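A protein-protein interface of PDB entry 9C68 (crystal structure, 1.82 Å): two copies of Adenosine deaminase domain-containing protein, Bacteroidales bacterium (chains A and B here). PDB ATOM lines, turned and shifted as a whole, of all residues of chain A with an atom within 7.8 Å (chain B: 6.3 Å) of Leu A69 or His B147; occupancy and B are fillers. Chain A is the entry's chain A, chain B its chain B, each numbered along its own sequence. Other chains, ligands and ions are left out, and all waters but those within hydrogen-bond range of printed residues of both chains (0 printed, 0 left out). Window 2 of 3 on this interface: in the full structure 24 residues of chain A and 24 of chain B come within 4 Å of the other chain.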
ATOM      1  N   LEU A  65     -23.825  -8.300  32.435  1.00  0.00           N
ATOM      2  CA  LEU A  65     -22.829  -9.307  32.093  1.00  0.00           C
ATOM      3  C   LEU A  65     -21.983  -9.611  33.322  1.00  0.00           C
ATOM      4  O   LEU A  65     -21.320  -8.715  33.864  1.00  0.00           O
ATOM      5  CB  LEU A  65     -21.944  -8.831  30.940  1.00  0.00           C
ATOM      6  CG  LEU A  65     -20.828  -9.771  30.483  1.00  0.00           C
ATOM      7  CD1 LEU A  65     -21.228 -11.252  30.496  1.00  0.00           C
ATOM      8  CD2 LEU A  65     -20.253  -9.328  29.162  1.00  0.00           C
ATOM      9  N   ALA A  66     -21.978 -10.873  33.738  1.00  0.00           N
ATOM     10  CA  ALA A  66     -21.247 -11.262  34.930  1.00  0.00           C
ATOM     11  C   ALA A  66     -20.002 -12.093  34.661  1.00  0.00           C
ATOM     12  O   ALA A  66     -19.032 -11.959  35.415  1.00  0.00           O
ATOM     13  CB  ALA A  66     -22.159 -12.042  35.886  1.00  0.00           C
ATOM     14  N   ASP A  67     -19.983 -12.943  33.612  1.00  0.00           N
ATOM     15  CA  ASP A  67     -18.919 -13.944  33.492  1.00  0.00           C
ATOM     16  C   ASP A  67     -18.082 -13.940  32.204  1.00  0.00           C
ATOM     17  O   ASP A  67     -16.923 -14.382  32.255  1.00  0.00           O
ATOM     18  CB  ASP A  67     -19.501 -15.344  33.694  1.00  0.00           C
ATOM     19  CG  ASP A  67     -19.831 -15.618  35.137  1.00  0.00           C
ATOM     20  OD1 ASP A  67     -19.044 -15.192  36.001  1.00  0.00           O
ATOM     21  OD2 ASP A  67     -20.868 -16.249  35.415  1.00  0.00           O
ATOM     22  N   ILE A  68     -18.595 -13.456  31.076  1.00  0.00           N
ATOM     23  CA  ILE A  68     -17.914 -13.600  29.778  1.00  0.00           C
ATOM     24  C   ILE A  68     -17.587 -15.057  29.488  1.00  0.00           C
ATOM     25  O   ILE A  68     -16.590 -15.602  29.978  1.00  0.00           O
ATOM     26  CB  ILE A  68     -16.621 -12.767  29.654  1.00  0.00           C
ATOM     27  CG1 ILE A  68     -16.850 -11.312  30.034  1.00  0.00           C
ATOM     28  CG2 ILE A  68     -16.118 -12.828  28.223  1.00  0.00           C
ATOM     29  CD1 ILE A  68     -15.541 -10.524  30.169  1.00  0.00           C
ATOM     30  N   LEU A  69     -18.419 -15.696  28.671  1.00  0.00           N
ATOM     31  CA  LEU A  69     -18.199 -17.062  28.236  1.00  0.00           C
ATOM     32  C   LEU A  69     -18.341 -17.227  26.728  1.00  0.00           C
ATOM     33  O   LEU A  69     -18.035 -18.312  26.219  1.00  0.00           O
ATOM     34  CB  LEU A  69     -19.182 -18.021  28.926  1.00  0.00           C
ATOM     35  CG  LEU A  69     -19.233 -17.973  30.452  1.00  0.00           C
ATOM     36  CD1 LEU A  69     -20.552 -18.564  30.949  1.00  0.00           C
ATOM     37  CD2 LEU A  69     -18.019 -18.666  31.058  1.00  0.00           C
ATOM     38  N   ASN A  70     -18.811 -16.198  26.013  1.00  0.00           N
ATOM     39  CA  ASN A  70     -19.062 -16.226  24.577  1.00  0.00           C
ATOM     40  C   ASN A  70     -18.313 -15.106  23.891  1.00  0.00           C
ATOM     41  O   ASN A  70     -17.961 -14.112  24.518  1.00  0.00           O
ATOM     42  CB  ASN A  70     -20.532 -15.996  24.198  1.00  0.00           C
ATOM     43  CG  ASN A  70     -21.456 -16.946  24.837  1.00  0.00           C
ATOM     44  OD1 ASN A  70     -21.330 -18.152  24.682  1.00  0.00           O
ATOM     45  ND2 ASN A  70     -22.488 -16.411  25.457  1.00  0.00           N
ATOM     46  N   GLU A  71     -18.146 -15.263  22.577  1.00  0.00           N
ATOM     47  CA  GLU A  71     -17.799 -14.164  21.693  1.00  0.00           C
ATOM     48  C   GLU A  71     -18.818 -13.057  21.877  1.00  0.00           C
ATOM     49  O   GLU A  71     -18.468 -11.886  21.935  1.00  0.00           O
ATOM     50  CB  GLU A  71     -17.779 -14.627  20.231  1.00  0.00           C
ATOM     51  CG  GLU A  71     -17.379 -13.551  19.233  1.00  0.00           C
ATOM     52  CD  GLU A  71     -17.363 -14.053  17.790  1.00  0.00           C
ATOM     53  OE1 GLU A  71     -17.713 -15.227  17.545  1.00  0.00           O
ATOM     54  OE2 GLU A  71     -16.998 -13.264  16.897  1.00  0.00           O
ATOM     55  N   ASP A  73     -16.584  -8.448  24.861  1.00  0.00           N
ATOM     56  CA  ASP A  73     -16.171  -9.746  24.354  1.00  0.00           C
ATOM     57  C   ASP A  73     -17.101 -10.875  24.723  1.00  0.00           C
ATOM     58  O   ASP A  73     -16.741 -12.004  24.441  1.00  0.00           O
ATOM     59  CB  ASP A  73     -14.761 -10.136  24.844  1.00  0.00           C
ATOM     60  CG  ASP A  73     -13.654  -9.679  23.903  1.00  0.00           C
ATOM     61  OD1 ASP A  73     -13.815  -9.885  22.691  1.00  0.00           O
ATOM     62  OD2 ASP A  73     -12.607  -9.152  24.381  1.00  0.00           O
ATOM     63  N   PHE A  74     -18.236 -10.611  25.383  1.00  0.00           N
ATOM     64  CA  PHE A  74     -19.354 -11.553  25.466  1.00  0.00           C
ATOM     65  C   PHE A  74     -20.500 -11.020  24.619  1.00  0.00           C
ATOM     66  O   PHE A  74     -21.654 -11.003  25.028  1.00  0.00           O
ATOM     67  CB  PHE A  74     -19.755 -11.759  26.925  1.00  0.00           C
ATOM     68  CG  PHE A  74     -20.834 -12.798  27.191  1.00  0.00           C
ATOM     69  CD1 PHE A  74     -22.185 -12.479  27.207  1.00  0.00           C
ATOM     70  CD2 PHE A  74     -20.476 -14.072  27.547  1.00  0.00           C
ATOM     71  CE1 PHE A  74     -23.123 -13.417  27.492  1.00  0.00           C
ATOM     72  CE2 PHE A  74     -21.395 -14.999  27.861  1.00  0.00           C
ATOM     73  CZ  PHE A  74     -22.732 -14.686  27.834  1.00  0.00           C
ATOM     74  N   GLU A  75     -20.164 -10.528  23.424  1.00  0.00           N
ATOM     75  CA  GLU A  75     -21.020  -9.651  22.640  1.00  0.00           C
ATOM     76  C   GLU A  75     -21.281  -8.312  23.335  1.00  0.00           C
ATOM     77  O   GLU A  75     -22.360  -7.734  23.149  1.00  0.00           O
ATOM     78  CB  GLU A  75     -22.343 -10.349  22.296  1.00  0.00           C
ATOM     79  CG  GLU A  75     -22.205 -11.476  21.291  1.00  0.00           C
ATOM     80  CD  GLU A  75     -22.282 -12.828  21.934  1.00  0.00           C
ATOM     81  OE1 GLU A  75     -21.531 -13.040  22.904  1.00  0.00           O
ATOM     82  OE2 GLU A  75     -23.086 -13.673  21.494  1.00  0.00           O
ATOM     83  N   ILE A 103     -10.696 -11.744  34.340  1.00  0.00           N
ATOM     84  CA  ILE A 103     -10.236 -12.906  33.589  1.00  0.00           C
ATOM     85  C   ILE A 103      -9.248 -12.398  32.552  1.00  0.00           C
ATOM     86  O   ILE A 103      -9.147 -11.187  32.338  1.00  0.00           O
ATOM     87  CB  ILE A 103     -11.395 -13.677  32.917  1.00  0.00           C
ATOM     88  CG1 ILE A 103     -12.052 -12.845  31.813  1.00  0.00           C
ATOM     89  CG2 ILE A 103     -12.419 -14.131  33.927  1.00  0.00           C
ATOM     90  CD1 ILE A 103     -12.932 -13.741  30.926  1.00  0.00           C
ATOM     91  N   HIS B 124      -9.605 -17.096  24.202  1.00  0.00           N
ATOM     92  CA  HIS B 124      -9.356 -17.554  25.569  1.00  0.00           C
ATOM     93  C   HIS B 124     -10.294 -18.722  25.881  1.00  0.00           C
ATOM     94  O   HIS B 124     -11.398 -18.808  25.339  1.00  0.00           O
ATOM     95  CB  HIS B 124      -9.558 -16.376  26.533  1.00  0.00           C
ATOM     96  CG  HIS B 124      -9.302 -16.685  27.975  1.00  0.00           C
ATOM     97  ND1 HIS B 124      -8.277 -17.501  28.399  1.00  0.00           N
ATOM     98  CD2 HIS B 124      -9.890 -16.208  29.096  1.00  0.00           C
ATOM     99  CE1 HIS B 124      -8.275 -17.551  29.720  1.00  0.00           C
ATOM    100  NE2 HIS B 124      -9.234 -16.764  30.168  1.00  0.00           N
ATOM    101  N   VAL B 125      -9.831 -19.645  26.719  1.00  0.00           N
ATOM    102  CA  VAL B 125     -10.590 -20.841  27.068  1.00  0.00           C
ATOM    103  C   VAL B 125     -10.877 -20.827  28.570  1.00  0.00           C
ATOM    104  O   VAL B 125      -9.964 -20.646  29.389  1.00  0.00           O
ATOM    105  CB  VAL B 125      -9.854 -22.122  26.629  1.00  0.00           C
ATOM    106  CG1 VAL B 125      -8.438 -22.137  27.108  1.00  0.00           C
ATOM    107  CG2 VAL B 125     -10.589 -23.348  27.120  1.00  0.00           C
ATOM    108  N   LEU B 126     -12.151 -20.967  28.920  1.00  0.00           N
ATOM    109  CA  LEU B 126     -12.601 -21.127  30.298  1.00  0.00           C
ATOM    110  C   LEU B 126     -13.181 -22.528  30.466  1.00  0.00           C
ATOM    111  O   LEU B 126     -13.974 -22.973  29.636  1.00  0.00           O
ATOM    112  CB  LEU B 126     -13.653 -20.068  30.645  1.00  0.00           C
ATOM    113  CG  LEU B 126     -13.236 -18.814  31.427  1.00  0.00           C
ATOM    114  CD1 LEU B 126     -12.188 -18.047  30.625  1.00  0.00           C
ATOM    115  CD2 LEU B 126     -14.445 -17.919  31.726  1.00  0.00           C
ATOM    116  N   ALA B 127     -12.785 -23.220  31.533  1.00  0.00           N
ATOM    117  CA  ALA B 127     -13.226 -24.578  31.819  1.00  0.00           C
ATOM    118  C   ALA B 127     -13.969 -24.599  33.149  1.00  0.00           C
ATOM    119  O   ALA B 127     -13.431 -24.134  34.156  1.00  0.00           O
ATOM    120  CB  ALA B 127     -12.018 -25.510  31.862  1.00  0.00           C
ATOM    121  N   ASP B 128     -15.194 -25.159  33.157  1.00  0.00           N
ATOM    122  CA  ASP B 128     -15.997 -25.212  34.384  1.00  0.00           C
ATOM    123  C   ASP B 128     -15.197 -25.769  35.554  1.00  0.00           C
ATOM    124  O   ASP B 128     -15.286 -25.261  36.678  1.00  0.00           O
ATOM    125  CB  ASP B 128     -17.259 -26.070  34.176  1.00  0.00           C
ATOM    126  CG  ASP B 128     -18.270 -25.423  33.236  1.00  0.00           C
ATOM    127  OD1 ASP B 128     -17.933 -24.430  32.576  1.00  0.00           O
ATOM    128  OD2 ASP B 128     -19.421 -25.902  33.143  1.00  0.00           O
ATOM    129  N   GLY B 144     -19.675 -30.258  27.294  1.00  0.00           N
ATOM    130  CA  GLY B 144     -19.754 -28.843  26.967  1.00  0.00           C
ATOM    131  C   GLY B 144     -19.318 -27.907  28.076  1.00  0.00           C
ATOM    132  O   GLY B 144     -19.887 -26.821  28.216  1.00  0.00           O
ATOM    133  N   GLN B 145     -18.347 -28.310  28.891  1.00  0.00           N
ATOM    134  CA  GLN B 145     -17.897 -27.504  30.027  1.00  0.00           C
ATOM    135  C   GLN B 145     -16.596 -26.764  29.734  1.00  0.00           C
ATOM    136  O   GLN B 145     -16.002 -26.194  30.658  1.00  0.00           O
ATOM    137  CB  GLN B 145     -17.742 -28.381  31.281  1.00  0.00           C
ATOM    138  CG  GLN B 145     -18.682 -29.566  31.291  1.00  0.00           C
ATOM    139  CD  GLN B 145     -18.773 -30.316  32.604  1.00  0.00           C
ATOM    140  OE1 GLN B 145     -17.812 -30.939  33.047  1.00  0.00           O
ATOM    141  NE2 GLN B 145     -19.963 -30.337  33.182  1.00  0.00           N
ATOM    142  N   ILE B 146     -16.115 -26.817  28.483  1.00  0.00           N
ATOM    143  CA  ILE B 146     -15.077 -25.921  27.960  1.00  0.00           C
ATOM    144  C   ILE B 146     -15.707 -24.840  27.101  1.00  0.00           C
ATOM    145  O   ILE B 146     -16.427 -25.145  26.143  1.00  0.00           O
ATOM    146  CB  ILE B 146     -14.017 -26.685  27.156  1.00  0.00           C
ATOM    147  CG1 ILE B 146     -13.516 -27.930  27.873  1.00  0.00           C
ATOM    148  CG2 ILE B 146     -12.915 -25.736  26.718  1.00  0.00           C
ATOM    149  CD1 ILE B 146     -13.381 -27.730  29.384  1.00  0.00           C
ATOM    150  N   HIS B 147     -15.412 -23.575  27.414  1.00  0.00           N
ATOM    151  CA  HIS B 147     -16.010 -22.446  26.715  1.00  0.00           C
ATOM    152  C   HIS B 147     -14.905 -21.676  26.023  1.00  0.00           C
ATOM    153  O   HIS B 147     -13.970 -21.204  26.672  1.00  0.00           O
ATOM    154  CB  HIS B 147     -16.773 -21.535  27.663  1.00  0.00           C
ATOM    155  CG  HIS B 147     -17.660 -22.274  28.607  1.00  0.00           C
ATOM    156  ND1 HIS B 147     -19.027 -22.325  28.454  1.00  0.00           N
ATOM    157  CD2 HIS B 147     -17.373 -23.009  29.705  1.00  0.00           C
ATOM    158  CE1 HIS B 147     -19.546 -23.055  29.424  1.00  0.00           C
ATOM    159  NE2 HIS B 147     -18.563 -23.477  30.200  1.00  0.00           N
ATOM    160  N   PHE B 148     -15.019 -21.556  24.716  1.00  0.00           N
ATOM    161  CA  PHE B 148     -14.066 -20.824  23.904  1.00  0.00           C
ATOM    162  C   PHE B 148     -14.612 -19.419  23.688  1.00  0.00           C
ATOM    163  O   PHE B 148     -15.753 -19.251  23.247  1.00  0.00           O
ATOM    164  CB  PHE B 148     -13.838 -21.570  22.591  1.00  0.00           C
ATOM    165  CG  PHE B 148     -13.147 -22.897  22.776  1.00  0.00           C
ATOM    166  CD1 PHE B 148     -11.778 -22.959  22.917  1.00  0.00           C
ATOM    167  CD2 PHE B 148     -13.876 -24.084  22.831  1.00  0.00           C
ATOM    168  CE1 PHE B 148     -11.131 -24.139  23.096  1.00  0.00           C
ATOM    169  CE2 PHE B 148     -13.230 -25.290  23.003  1.00  0.00           C
ATOM    170  CZ  PHE B 148     -11.849 -25.322  23.144  1.00  0.00           C
ATOM    171  N   ILE B 149     -13.822 -18.414  24.055  1.00  0.00           N
ATOM    172  CA  ILE B 149     -14.185 -17.010  23.893  1.00  0.00           C
ATOM    173  C   ILE B 149     -13.405 -16.467  22.705  1.00  0.00           C
ATOM    174  O   ILE B 149     -12.184 -16.282  22.788  1.00  0.00           O
ATOM    175  CB  ILE B 149     -13.896 -16.193  25.160  1.00  0.00           C
ATOM    176  CG1 ILE B 149     -14.495 -16.886  26.396  1.00  0.00           C
ATOM    177  CG2 ILE B 149     -14.373 -14.761  25.013  1.00  0.00           C
ATOM    178  CD1 ILE B 149     -13.861 -16.486  27.707  1.00  0.00           C
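The backbone NH (N) of Ile B149 sits at hydrogen-bond distance from the backbone carbonyl oxygen (O) of His B124, 2.8 Å away.
The side-chain carboxylate of Asp B128 is in hydrogen-bond range of a ring nitrogen (NE2) of His B147.
The backbone NH (N) of His B147 lies within hydrogen-bond range of the backbone carbonyl oxygen (O) of Leu B126, 2.7 Å away.
Among the printed residues, pairs that only touch across the chains: Ile A68 with Leu B126, Ile A68 with Ile B149, Asp A73 with Ile B149, Asn A70 with Ile B149, Leu A69 with Leu B126, Leu A69 with His B147, Leu A69 with Ile B149 and Leu A69 with Phe B148.
Of the printed residues of chain B, Ile A68 touches Leu B126 and Ile B149.
Of the printed residues of chain A, Leu B126 touches Ile A68 (3.6 Å) and Leu A69 (3.7 Å).
Of chain A, only Leu A69 (3.8 Å) comes within 4 Å of His B147.
Of the 11 printed residues of chain B, 4 touch a printed residue of chain A.
Of the 11 printed residues of chain A, 4 touch a printed residue of chain B.
Hydrophobic or aromatic side chains of chain A that line the printed part of chain B: Leu A69.
Among the printed residues, 8 pairs touch across the chains.
Among the printed residues, no Asp or Glu carboxylate lies within 4 Å of a Lys or Arg side-chain nitrogen of the other chain.
No position is printed for both chains.
Of the 8 pairs that touch across the chains among the printed residues, none has its exchanged pair printed and touching as well.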
